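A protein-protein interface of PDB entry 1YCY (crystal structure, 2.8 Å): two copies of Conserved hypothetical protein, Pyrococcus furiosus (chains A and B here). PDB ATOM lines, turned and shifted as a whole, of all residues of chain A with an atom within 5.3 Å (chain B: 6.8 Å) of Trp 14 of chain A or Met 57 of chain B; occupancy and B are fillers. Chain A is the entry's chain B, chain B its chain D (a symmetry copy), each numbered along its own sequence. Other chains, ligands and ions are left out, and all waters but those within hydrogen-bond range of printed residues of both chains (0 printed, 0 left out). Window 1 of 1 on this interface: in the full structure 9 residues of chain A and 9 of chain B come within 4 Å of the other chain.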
ATOM      1  N   VAL A  10      -3.489 -25.257  15.330  1.00  0.00           N
ATOM      2  CA  VAL A  10      -4.070 -25.773  14.100  1.00  0.00           C
ATOM      3  C   VAL A  10      -3.924 -24.765  12.966  1.00  0.00           C
ATOM      4  O   VAL A  10      -3.583 -25.111  11.836  1.00  0.00           O
ATOM      5  CB  VAL A  10      -5.548 -26.120  14.306  1.00  0.00           C
ATOM      6  CG1 VAL A  10      -6.174 -26.629  13.009  1.00  0.00           C
ATOM      7  CG2 VAL A  10      -5.683 -27.164  15.405  1.00  0.00           C
ATOM      8  N   LEU A  11      -4.189 -23.507  13.272  1.00  0.00           N
ATOM      9  CA  LEU A  11      -4.130 -22.469  12.263  1.00  0.00           C
ATOM     10  C   LEU A  11      -2.704 -22.333  11.739  1.00  0.00           C
ATOM     11  O   LEU A  11      -2.498 -22.202  10.526  1.00  0.00           O
ATOM     12  CB  LEU A  11      -4.671 -21.144  12.819  1.00  0.00           C
ATOM     13  CG  LEU A  11      -6.207 -21.074  12.982  1.00  0.00           C
ATOM     14  CD1 LEU A  11      -6.573 -19.811  13.691  1.00  0.00           C
ATOM     15  CD2 LEU A  11      -6.933 -21.155  11.643  1.00  0.00           C
ATOM     16  N   LYS A  12      -1.721 -22.408  12.643  1.00  0.00           N
ATOM     17  CA  LYS A  12      -0.310 -22.513  12.228  1.00  0.00           C
ATOM     18  C   LYS A  12      -0.163 -23.588  11.143  1.00  0.00           C
ATOM     19  O   LYS A  12       0.358 -23.314  10.070  1.00  0.00           O
ATOM     20  CB  LYS A  12       0.611 -22.853  13.415  1.00  0.00           C
ATOM     21  CG  LYS A  12       0.671 -21.812  14.541  1.00  0.00           C
ATOM     22  N   GLU A  13      -0.649 -24.796  11.422  1.00  0.00           N
ATOM     23  CA  GLU A  13      -0.513 -25.919  10.485  1.00  0.00           C
ATOM     24  C   GLU A  13      -1.248 -25.663   9.196  1.00  0.00           C
ATOM     25  O   GLU A  13      -0.847 -26.154   8.142  1.00  0.00           O
ATOM     26  CB  GLU A  13      -1.087 -27.204  11.069  1.00  0.00           C
ATOM     27  CG  GLU A  13      -0.492 -27.665  12.384  1.00  0.00           C
ATOM     28  CD  GLU A  13      -1.391 -28.656  13.098  1.00  0.00           C
ATOM     29  OE1 GLU A  13      -1.288 -28.748  14.342  1.00  0.00           O
ATOM     30  OE2 GLU A  13      -2.209 -29.330  12.412  1.00  0.00           O
ATOM     31  N   TRP A  14      -2.350 -24.927   9.292  1.00  0.00           N
ATOM     32  CA  TRP A  14      -3.209 -24.657   8.132  1.00  0.00           C
ATOM     33  C   TRP A  14      -2.692 -23.504   7.270  1.00  0.00           C
ATOM     34  O   TRP A  14      -3.130 -23.330   6.106  1.00  0.00           O
ATOM     35  CB  TRP A  14      -4.626 -24.322   8.595  1.00  0.00           C
ATOM     36  CG  TRP A  14      -5.402 -25.486   9.133  1.00  0.00           C
ATOM     37  CD1 TRP A  14      -4.916 -26.714   9.518  1.00  0.00           C
ATOM     38  CD2 TRP A  14      -6.815 -25.519   9.384  1.00  0.00           C
ATOM     39  NE1 TRP A  14      -5.945 -27.505   9.969  1.00  0.00           N
ATOM     40  CE2 TRP A  14      -7.119 -26.798   9.898  1.00  0.00           C
ATOM     41  CE3 TRP A  14      -7.855 -24.593   9.216  1.00  0.00           C
ATOM     42  CZ2 TRP A  14      -8.415 -27.169  10.252  1.00  0.00           C
ATOM     43  CZ3 TRP A  14      -9.138 -24.968   9.561  1.00  0.00           C
ATOM     44  CH2 TRP A  14      -9.408 -26.245  10.072  1.00  0.00           C
ATOM     45  N   LYS A  15      -1.786 -22.708   7.853  1.00  0.00           N
ATOM     46  CA  LYS A  15      -1.229 -21.538   7.181  1.00  0.00           C
ATOM     47  C   LYS A  15      -0.578 -21.965   5.878  1.00  0.00           C
ATOM     48  O   LYS A  15       0.299 -22.819   5.874  1.00  0.00           O
ATOM     49  CB  LYS A  15      -0.224 -20.822   8.079  1.00  0.00           C
ATOM     50  CG  LYS A  15      -0.024 -19.385   7.676  1.00  0.00           C
ATOM     51  CD  LYS A  15       0.967 -18.673   8.577  1.00  0.00           C
ATOM     52  CE  LYS A  15       0.408 -18.478   9.982  1.00  0.00           C
ATOM     53  NZ  LYS A  15       1.195 -17.480  10.797  1.00  0.00           N
ATOM     54  N   GLY A  16      -1.055 -21.395   4.779  1.00  0.00           N
ATOM     55  CA  GLY A  16      -0.588 -21.747   3.450  1.00  0.00           C
ATOM     56  C   GLY A  16      -1.579 -22.580   2.663  1.00  0.00           C
ATOM     57  O   GLY A  16      -1.628 -22.509   1.426  1.00  0.00           O
ATOM     58  N   HIS A  17      -2.372 -23.378   3.374  1.00  0.00           N
ATOM     59  CA  HIS A  17      -3.302 -24.287   2.719  1.00  0.00           C
ATOM     60  C   HIS A  17      -4.599 -23.594   2.415  1.00  0.00           C
ATOM     61  O   HIS A  17      -4.993 -22.666   3.111  1.00  0.00           O
ATOM     62  CB  HIS A  17      -3.537 -25.522   3.572  1.00  0.00           C
ATOM     63  CG  HIS A  17      -2.292 -26.321   3.811  1.00  0.00           C
ATOM     64  ND1 HIS A  17      -1.663 -26.377   5.042  1.00  0.00           N
ATOM     65  CD2 HIS A  17      -1.534 -27.061   2.964  1.00  0.00           C
ATOM     66  CE1 HIS A  17      -0.585 -27.132   4.946  1.00  0.00           C
ATOM     67  NE2 HIS A  17      -0.482 -27.556   3.696  1.00  0.00           N
ATOM     68  N   LYS A  18      -5.241 -24.036   1.344  1.00  0.00           N
ATOM     69  CA  LYS A  18      -6.568 -23.579   0.981  1.00  0.00           C
ATOM     70  C   LYS A  18      -7.568 -23.959   2.088  1.00  0.00           C
ATOM     71  O   LYS A  18      -7.560 -25.093   2.582  1.00  0.00           O
ATOM     72  CB  LYS A  18      -6.982 -24.204  -0.350  1.00  0.00           C
ATOM     73  CG  LYS A  18      -8.297 -23.710  -0.890  1.00  0.00           C
ATOM     74  CD  LYS A  18      -8.602 -24.282  -2.280  1.00  0.00           C
ATOM     75  CE  LYS A  18      -9.972 -23.799  -2.785  1.00  0.00           C
ATOM     76  NZ  LYS A  18     -10.392 -24.423  -4.094  1.00  0.00           N
ATOM     77  N   VAL A  19      -8.387 -22.984   2.488  1.00  0.00           N
ATOM     78  CA  VAL A  19      -9.372 -23.149   3.538  1.00  0.00           C
ATOM     79  C   VAL A  19     -10.684 -22.522   3.101  1.00  0.00           C
ATOM     80  O   VAL A  19     -10.674 -21.556   2.339  1.00  0.00           O
ATOM     81  CB  VAL A  19      -8.924 -22.495   4.860  1.00  0.00           C
ATOM     82  CG1 VAL A  19      -7.546 -22.944   5.211  1.00  0.00           C
ATOM     83  CG2 VAL A  19      -8.969 -20.976   4.785  1.00  0.00           C
ATOM     84  N   LEU A  33      -5.118 -19.581   3.639  1.00  0.00           N
ATOM     85  CA  LEU A  33      -4.933 -18.933   4.924  1.00  0.00           C
ATOM     86  C   LEU A  33      -3.563 -18.334   4.893  1.00  0.00           C
ATOM     87  O   LEU A  33      -2.550 -19.015   5.090  1.00  0.00           O
ATOM     88  CB  LEU A  33      -5.045 -19.896   6.105  1.00  0.00           C
ATOM     89  CG  LEU A  33      -4.659 -19.241   7.448  1.00  0.00           C
ATOM     90  CD1 LEU A  33      -5.637 -18.116   7.817  1.00  0.00           C
ATOM     91  CD2 LEU A  33      -4.581 -20.236   8.577  1.00  0.00           C
ATOM     92  N   TRP A  66     -17.348 -21.421  11.489  1.00  0.00           N
ATOM     93  CA  TRP A  66     -16.387 -22.476  11.406  1.00  0.00           C
ATOM     94  C   TRP A  66     -15.413 -22.235  10.275  1.00  0.00           C
ATOM     95  O   TRP A  66     -15.780 -21.711   9.222  1.00  0.00           O
ATOM     96  CB  TRP A  66     -17.097 -23.814  11.209  1.00  0.00           C
ATOM     97  CG  TRP A  66     -18.077 -23.853  10.099  1.00  0.00           C
ATOM     98  CD1 TRP A  66     -19.416 -23.829  10.222  1.00  0.00           C
ATOM     99  CD2 TRP A  66     -17.804 -23.963   8.692  1.00  0.00           C
ATOM    100  NE1 TRP A  66     -20.016 -23.915   8.986  1.00  0.00           N
ATOM    101  CE2 TRP A  66     -19.052 -23.992   8.029  1.00  0.00           C
ATOM    102  CE3 TRP A  66     -16.638 -24.028   7.934  1.00  0.00           C
ATOM    103  CZ2 TRP A  66     -19.170 -24.084   6.658  1.00  0.00           C
ATOM    104  CZ3 TRP A  66     -16.755 -24.124   6.574  1.00  0.00           C
ATOM    105  CH2 TRP A  66     -18.020 -24.150   5.943  1.00  0.00           C
ATOM    106  N   ILE A  67     -14.170 -22.640  10.501  1.00  0.00           N
ATOM    107  CA  ILE A  67     -13.169 -22.678   9.447  1.00  0.00           C
ATOM    108  C   ILE A  67     -12.882 -24.115   9.125  1.00  0.00           C
ATOM    109  O   ILE A  67     -12.918 -24.981   9.992  1.00  0.00           O
ATOM    110  CB  ILE A  67     -11.841 -22.053   9.870  1.00  0.00           C
ATOM    111  CG1 ILE A  67     -12.062 -20.795  10.708  1.00  0.00           C
ATOM    112  CG2 ILE A  67     -11.031 -21.728   8.650  1.00  0.00           C
ATOM    113  CD1 ILE A  67     -10.958 -20.521  11.720  1.00  0.00           C
ATOM    114  N   MET A  68     -12.533 -24.359   7.888  1.00  0.00           N
ATOM    115  CA  MET A  68     -12.357 -25.689   7.450  1.00  0.00           C
ATOM    116  C   MET A  68     -11.256 -25.820   6.410  1.00  0.00           C
ATOM    117  O   MET A  68     -11.332 -25.246   5.326  1.00  0.00           O
ATOM    118  CB  MET A  68     -13.657 -26.119   6.865  1.00  0.00           C
ATOM    119  CG  MET A  68     -13.537 -27.284   5.994  1.00  0.00           C
ATOM    120  SD  MET A  68     -15.261 -27.822   5.495  1.00  0.00           S
ATOM    121  CE  MET A  68     -15.657 -26.448   4.155  1.00  0.00           C
ATOM    122  N   LEU A  69     -10.247 -26.616   6.748  1.00  0.00           N
ATOM    123  CA  LEU A  69      -9.163 -26.960   5.827  1.00  0.00           C
ATOM    124  C   LEU A  69      -9.655 -27.898   4.748  1.00  0.00           C
ATOM    125  O   LEU A  69     -10.153 -28.956   5.055  1.00  0.00           O
ATOM    126  CB  LEU A  69      -8.026 -27.629   6.604  1.00  0.00           C
ATOM    127  CG  LEU A  69      -6.966 -28.419   5.838  1.00  0.00           C
ATOM    128  CD1 LEU A  69      -6.434 -27.647   4.629  1.00  0.00           C
ATOM    129  CD2 LEU A  69      -5.844 -28.774   6.806  1.00  0.00           C
ATOM    130  N   VAL B  21     -22.627 -32.337  15.102  1.00  0.00           N
ATOM    131  CA  VAL B  21     -22.587 -31.063  15.814  1.00  0.00           C
ATOM    132  C   VAL B  21     -23.577 -30.081  15.203  1.00  0.00           C
ATOM    133  O   VAL B  21     -23.766 -30.044  13.968  1.00  0.00           O
ATOM    134  CB  VAL B  21     -21.172 -30.447  15.785  1.00  0.00           C
ATOM    135  CG1 VAL B  21     -20.986 -29.477  16.939  1.00  0.00           C
ATOM    136  CG2 VAL B  21     -20.107 -31.531  15.865  1.00  0.00           C
ATOM    137  N   VAL B  23     -24.169 -26.119  14.973  1.00  0.00           N
ATOM    138  CA  VAL B  23     -23.606 -24.761  15.102  1.00  0.00           C
ATOM    139  C   VAL B  23     -24.650 -23.748  14.601  1.00  0.00           C
ATOM    140  O   VAL B  23     -24.836 -23.595  13.389  1.00  0.00           O
ATOM    141  CB  VAL B  23     -22.310 -24.605  14.273  1.00  0.00           C
ATOM    142  N   PHE B  29     -23.365 -30.810   9.940  1.00  0.00           N
ATOM    143  CA  PHE B  29     -22.014 -31.373   9.741  1.00  0.00           C
ATOM    144  C   PHE B  29     -21.638 -32.465  10.730  1.00  0.00           C
ATOM    145  O   PHE B  29     -21.860 -32.338  11.942  1.00  0.00           O
ATOM    146  CB  PHE B  29     -20.942 -30.263   9.792  1.00  0.00           C
ATOM    147  CG  PHE B  29     -20.889 -29.438   8.544  1.00  0.00           C
ATOM    148  CD1 PHE B  29     -20.609 -30.041   7.313  1.00  0.00           C
ATOM    149  CD2 PHE B  29     -21.163 -28.075   8.582  1.00  0.00           C
ATOM    150  CE1 PHE B  29     -20.585 -29.292   6.132  1.00  0.00           C
ATOM    151  CE2 PHE B  29     -21.149 -27.310   7.406  1.00  0.00           C
ATOM    152  CZ  PHE B  29     -20.854 -27.920   6.175  1.00  0.00           C
ATOM    153  N   THR B  30     -21.031 -33.524  10.203  1.00  0.00           N
ATOM    154  CA  THR B  30     -20.471 -34.599  11.046  1.00  0.00           C
ATOM    155  C   THR B  30     -19.003 -34.982  10.687  1.00  0.00           C
ATOM    156  O   THR B  30     -18.544 -34.813   9.543  1.00  0.00           O
ATOM    157  CB  THR B  30     -21.374 -35.877  10.997  1.00  0.00           C
ATOM    158  OG1 THR B  30     -21.046 -36.739  12.094  1.00  0.00           O
ATOM    159  CG2 THR B  30     -21.200 -36.635   9.678  1.00  0.00           C
ATOM    160  N   ILE B  41     -13.438 -27.079  19.231  1.00  0.00           N
ATOM    161  CA  ILE B  41     -13.244 -28.469  18.895  1.00  0.00           C
ATOM    162  C   ILE B  41     -12.848 -28.599  17.426  1.00  0.00           C
ATOM    163  O   ILE B  41     -13.214 -27.771  16.576  1.00  0.00           O
ATOM    164  CB  ILE B  41     -14.488 -29.340  19.152  1.00  0.00           C
ATOM    165  CG1 ILE B  41     -15.499 -29.158  18.026  1.00  0.00           C
ATOM    166  CG2 ILE B  41     -15.091 -29.048  20.525  1.00  0.00           C
ATOM    167  CD1 ILE B  41     -16.792 -29.784  18.291  1.00  0.00           C
ATOM    168  N   LEU B  42     -12.115 -29.672  17.141  1.00  0.00           N
ATOM    169  CA  LEU B  42     -11.562 -29.903  15.832  1.00  0.00           C
ATOM    170  C   LEU B  42     -12.019 -31.255  15.339  1.00  0.00           C
ATOM    171  O   LEU B  42     -11.989 -32.214  16.085  1.00  0.00           O
ATOM    172  CB  LEU B  42     -10.037 -29.851  15.927  1.00  0.00           C
ATOM    173  CG  LEU B  42      -9.247 -30.462  14.769  1.00  0.00           C
ATOM    174  CD1 LEU B  42      -9.358 -29.593  13.501  1.00  0.00           C
ATOM    175  CD2 LEU B  42      -7.805 -30.684  15.226  1.00  0.00           C
ATOM    176  N   LEU B  43     -12.421 -31.323  14.081  1.00  0.00           N
ATOM    177  CA  LEU B  43     -12.979 -32.532  13.507  1.00  0.00           C
ATOM    178  C   LEU B  43     -12.126 -33.023  12.352  1.00  0.00           C
ATOM    179  O   LEU B  43     -11.630 -32.235  11.589  1.00  0.00           O
ATOM    180  CB  LEU B  43     -14.407 -32.267  12.992  1.00  0.00           C
ATOM    181  CG  LEU B  43     -15.540 -32.554  13.969  1.00  0.00           C
ATOM    182  CD1 LEU B  43     -15.314 -31.803  15.261  1.00  0.00           C
ATOM    183  CD2 LEU B  43     -16.889 -32.211  13.351  1.00  0.00           C
ATOM    184  N   LYS B  44     -11.978 -34.335  12.218  1.00  0.00           N
ATOM    185  CA  LYS B  44     -11.327 -34.933  11.056  1.00  0.00           C
ATOM    186  C   LYS B  44     -12.390 -35.533  10.138  1.00  0.00           C
ATOM    187  O   LYS B  44     -13.537 -35.727  10.534  1.00  0.00           O
ATOM    188  CB  LYS B  44     -10.349 -36.009  11.515  1.00  0.00           C
ATOM    189  N   ASP B  45     -12.021 -35.815   8.902  1.00  0.00           N
ATOM    190  CA  ASP B  45     -12.897 -36.580   7.991  1.00  0.00           C
ATOM    191  C   ASP B  45     -14.354 -36.061   7.919  1.00  0.00           C
ATOM    192  O   ASP B  45     -15.290 -36.831   8.075  1.00  0.00           O
ATOM    193  CB  ASP B  45     -12.902 -38.068   8.416  1.00  0.00           C
ATOM    194  CG  ASP B  45     -11.660 -38.824   7.952  1.00  0.00           C
ATOM    195  OD1 ASP B  45     -11.551 -39.060   6.724  1.00  0.00           O
ATOM    196  OD2 ASP B  45     -10.815 -39.197   8.808  1.00  0.00           O
ATOM    197  N   VAL B  46     -14.542 -34.769   7.658  1.00  0.00           N
ATOM    198  CA  VAL B  46     -15.867 -34.164   7.773  1.00  0.00           C
ATOM    199  C   VAL B  46     -16.715 -34.444   6.552  1.00  0.00           C
ATOM    200  O   VAL B  46     -16.282 -34.202   5.436  1.00  0.00           O
ATOM    201  CB  VAL B  46     -15.782 -32.652   8.008  1.00  0.00           C
ATOM    202  CG1 VAL B  46     -17.170 -32.006   7.923  1.00  0.00           C
ATOM    203  CG2 VAL B  46     -15.132 -32.377   9.372  1.00  0.00           C
ATOM    204  N   GLY B  54     -14.204 -31.841   4.045  1.00  0.00           N
ATOM    205  CA  GLY B  54     -12.917 -31.236   4.354  1.00  0.00           C
ATOM    206  C   GLY B  54     -12.084 -32.018   5.330  1.00  0.00           C
ATOM    207  O   GLY B  54     -12.602 -32.574   6.296  1.00  0.00           O
ATOM    208  N   LYS B  55     -10.776 -32.047   5.077  1.00  0.00           N
ATOM    209  CA  LYS B  55      -9.862 -32.840   5.881  1.00  0.00           C
ATOM    210  C   LYS B  55     -10.139 -32.537   7.346  1.00  0.00           C
ATOM    211  O   LYS B  55     -10.295 -33.445   8.149  1.00  0.00           O
ATOM    212  CB  LYS B  55      -8.376 -32.560   5.535  1.00  0.00           C
ATOM    213  CG  LYS B  55      -7.982 -32.625   4.045  1.00  0.00           C
ATOM    214  N   GLN B  56     -10.242 -31.257   7.682  1.00  0.00           N
ATOM    215  CA  GLN B  56     -10.462 -30.854   9.067  1.00  0.00           C
ATOM    216  C   GLN B  56     -11.488 -29.718   9.175  1.00  0.00           C
ATOM    217  O   GLN B  56     -11.965 -29.194   8.163  1.00  0.00           O
ATOM    218  CB  GLN B  56      -9.137 -30.447   9.738  1.00  0.00           C
ATOM    219  CG  GLN B  56      -8.006 -31.503   9.715  1.00  0.00           C
ATOM    220  CD  GLN B  56      -6.844 -31.148  10.663  1.00  0.00           C
ATOM    221  OE1 GLN B  56      -6.993 -31.206  11.877  1.00  0.00           O
ATOM    222  NE2 GLN B  56      -5.695 -30.792  10.103  1.00  0.00           N
ATOM    223  N   MET B  57     -11.832 -29.367  10.412  1.00  0.00           N
ATOM    224  CA  MET B  57     -12.770 -28.305  10.665  1.00  0.00           C
ATOM    225  C   MET B  57     -12.685 -27.805  12.073  1.00  0.00           C
ATOM    226  O   MET B  57     -12.758 -28.575  13.014  1.00  0.00           O
ATOM    227  CB  MET B  57     -14.159 -28.806  10.433  1.00  0.00           C
ATOM    228  CG  MET B  57     -15.202 -28.009  11.156  1.00  0.00           C
ATOM    229  SD  MET B  57     -16.722 -27.901  10.034  1.00  0.00           S
ATOM    230  CE  MET B  57     -18.211 -27.672  11.350  1.00  0.00           C
ATOM    231  N   LEU B  58     -12.557 -26.494  12.208  1.00  0.00           N
ATOM    232  CA  LEU B  58     -12.569 -25.855  13.510  1.00  0.00           C
ATOM    233  C   LEU B  58     -13.931 -25.237  13.758  1.00  0.00           C
ATOM    234  O   LEU B  58     -14.580 -24.738  12.858  1.00  0.00           O
ATOM    235  CB  LEU B  58     -11.492 -24.774  13.592  1.00  0.00           C
ATOM    236  CG  LEU B  58     -10.048 -25.184  13.919  1.00  0.00           C
ATOM    237  CD1 LEU B  58      -9.101 -24.002  13.666  1.00  0.00           C
ATOM    238  CD2 LEU B  58      -9.922 -25.652  15.356  1.00  0.00           C
ATOM    239  N   ILE B  59     -14.354 -25.285  15.005  1.00  0.00           N
ATOM    240  CA  ILE B  59     -15.663 -24.810  15.411  1.00  0.00           C
ATOM    241  C   ILE B  59     -15.519 -24.381  16.848  1.00  0.00           C
ATOM    242  O   ILE B  59     -14.973 -25.136  17.647  1.00  0.00           O
ATOM    243  CB  ILE B  59     -16.695 -25.927  15.384  1.00  0.00           C
ATOM    244  CG1 ILE B  59     -16.430 -26.889  14.225  1.00  0.00           C
ATOM    245  CG2 ILE B  59     -18.072 -25.356  15.295  1.00  0.00           C
ATOM    246  CD1 ILE B  59     -17.232 -28.140  14.309  1.00  0.00           C
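The side-chain amide nitrogen (NE2) of Gln 56 of chain B sits close to the indole nitrogen (NE1) of Trp 14 of chain A (3.3 Å).
The backbone carbonyl oxygen (O) of Ile 67 of chain A is in hydrogen-bond range of the backbone NH (N) of Leu 58 of chain B (2.7 Å).
The backbone carbonyl oxygen of Leu 69 of chain A is in hydrogen-bond range of the backbone NH of Lys 55 of chain B, 3.2 Å away.
The backbone carbonyl oxygen of Gln 56 of chain B sits at hydrogen-bond distance from the backbone NH of Leu 69 of chain A (3.4 Å).
No position is printed for both chains.
The backbone carbonyl oxygen (O) of Phe 29 of chain B lies within hydrogen-bond range of the backbone NH (N) of Val 21 of chain B (3.3 Å).
The backbone NH (N) of Leu 43 of chain B lies within hydrogen-bond range of the backbone carbonyl oxygen (O) of Met 57 of chain B.
The backbone NH of Asp 45 of chain B sits at hydrogen-bond distance from the backbone carbonyl oxygen of Lys 55 of chain B (3.0 Å).
The backbone carbonyl oxygen (O) of Gly 54 of chain B lies within hydrogen-bond range of the backbone NH (N) of Val 46 of chain B (3.2 Å).
Among the printed residues, merely in contact across the chains: Trp 66 of chain A with Leu 58 of chain B, Met 68 of chain A with Gln 56 of chain B, Ile 67 of chain A with Met 57 of chain B, Leu 69 of chain A with Gly 54 of chain B, Trp 14 of chain A with Leu 58 of chain B, Trp 66 of chain A with Phe 29 of chain B, Trp 14 of chain A with Met 57 of chain B and Val 10 of chain A with Leu 58 of chain B.
Printed residues of chain B within 4 Å of Val 10 of chain A: Leu 58 (3.99 Å).
Lys 12 of chain A touches none of the printed residues of chain B.
Trp 14 of chain A touches just these residues of chain B: Gln 56 (3.3 Å), Met 57 (3.97 Å) and Leu 58 (3.8 Å).
Printed residues of chain B within 4 Å of Trp 66 of chain A: Phe 29 (3.9 Å) and Leu 58 (3.1 Å).
Printed residues of chain B within 4 Å of Met 68 of chain A: Gln 56.
Printed residues of chain B within 4 Å of Leu 69 of chain A: Gly 54 (3.6 Å), Lys 55 (3.2 Å) and Gln 56 (3.4 Å).
Of the printed residues of chain A, Phe 29 of chain B touches Trp 66 (3.9 Å).
Of the printed residues of chain A, Met 57 of chain B touches Trp 14 (3.97 Å) and Ile 67 (3.4 Å).
The nearest residue of chain B that does not touch Trp 14 of chain A is Leu 42 of chain B (4.2 Å).
The nearest printed residue of chain A that does not touch Met 57 of chain B is Trp 66 of chain A (4.02 Å).
Printed residues of chain A that touch a printed residue of chain B: Val 10, Trp 14, Trp 66, Ile 67, Met 68 and Leu 69.
Hydrophobic or aromatic side chains of chain A that line the printed part of chain B: Val 10, Trp 14, Trp 66, Met 68 and Leu 69.
Of the 16 printed residues of chain B, 6 touch a printed residue of chain A.
Hydrophobic or aromatic side chains of chain B that line the printed part of chain A: Phe 29, Met 57 and Leu 58.
Among the printed residues, 12 pairs touch across the chains.
Among the printed residues, no Asp or Glu carboxylate lies within 4 Å of a Lys or Arg side-chain nitrogen of the other chain.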
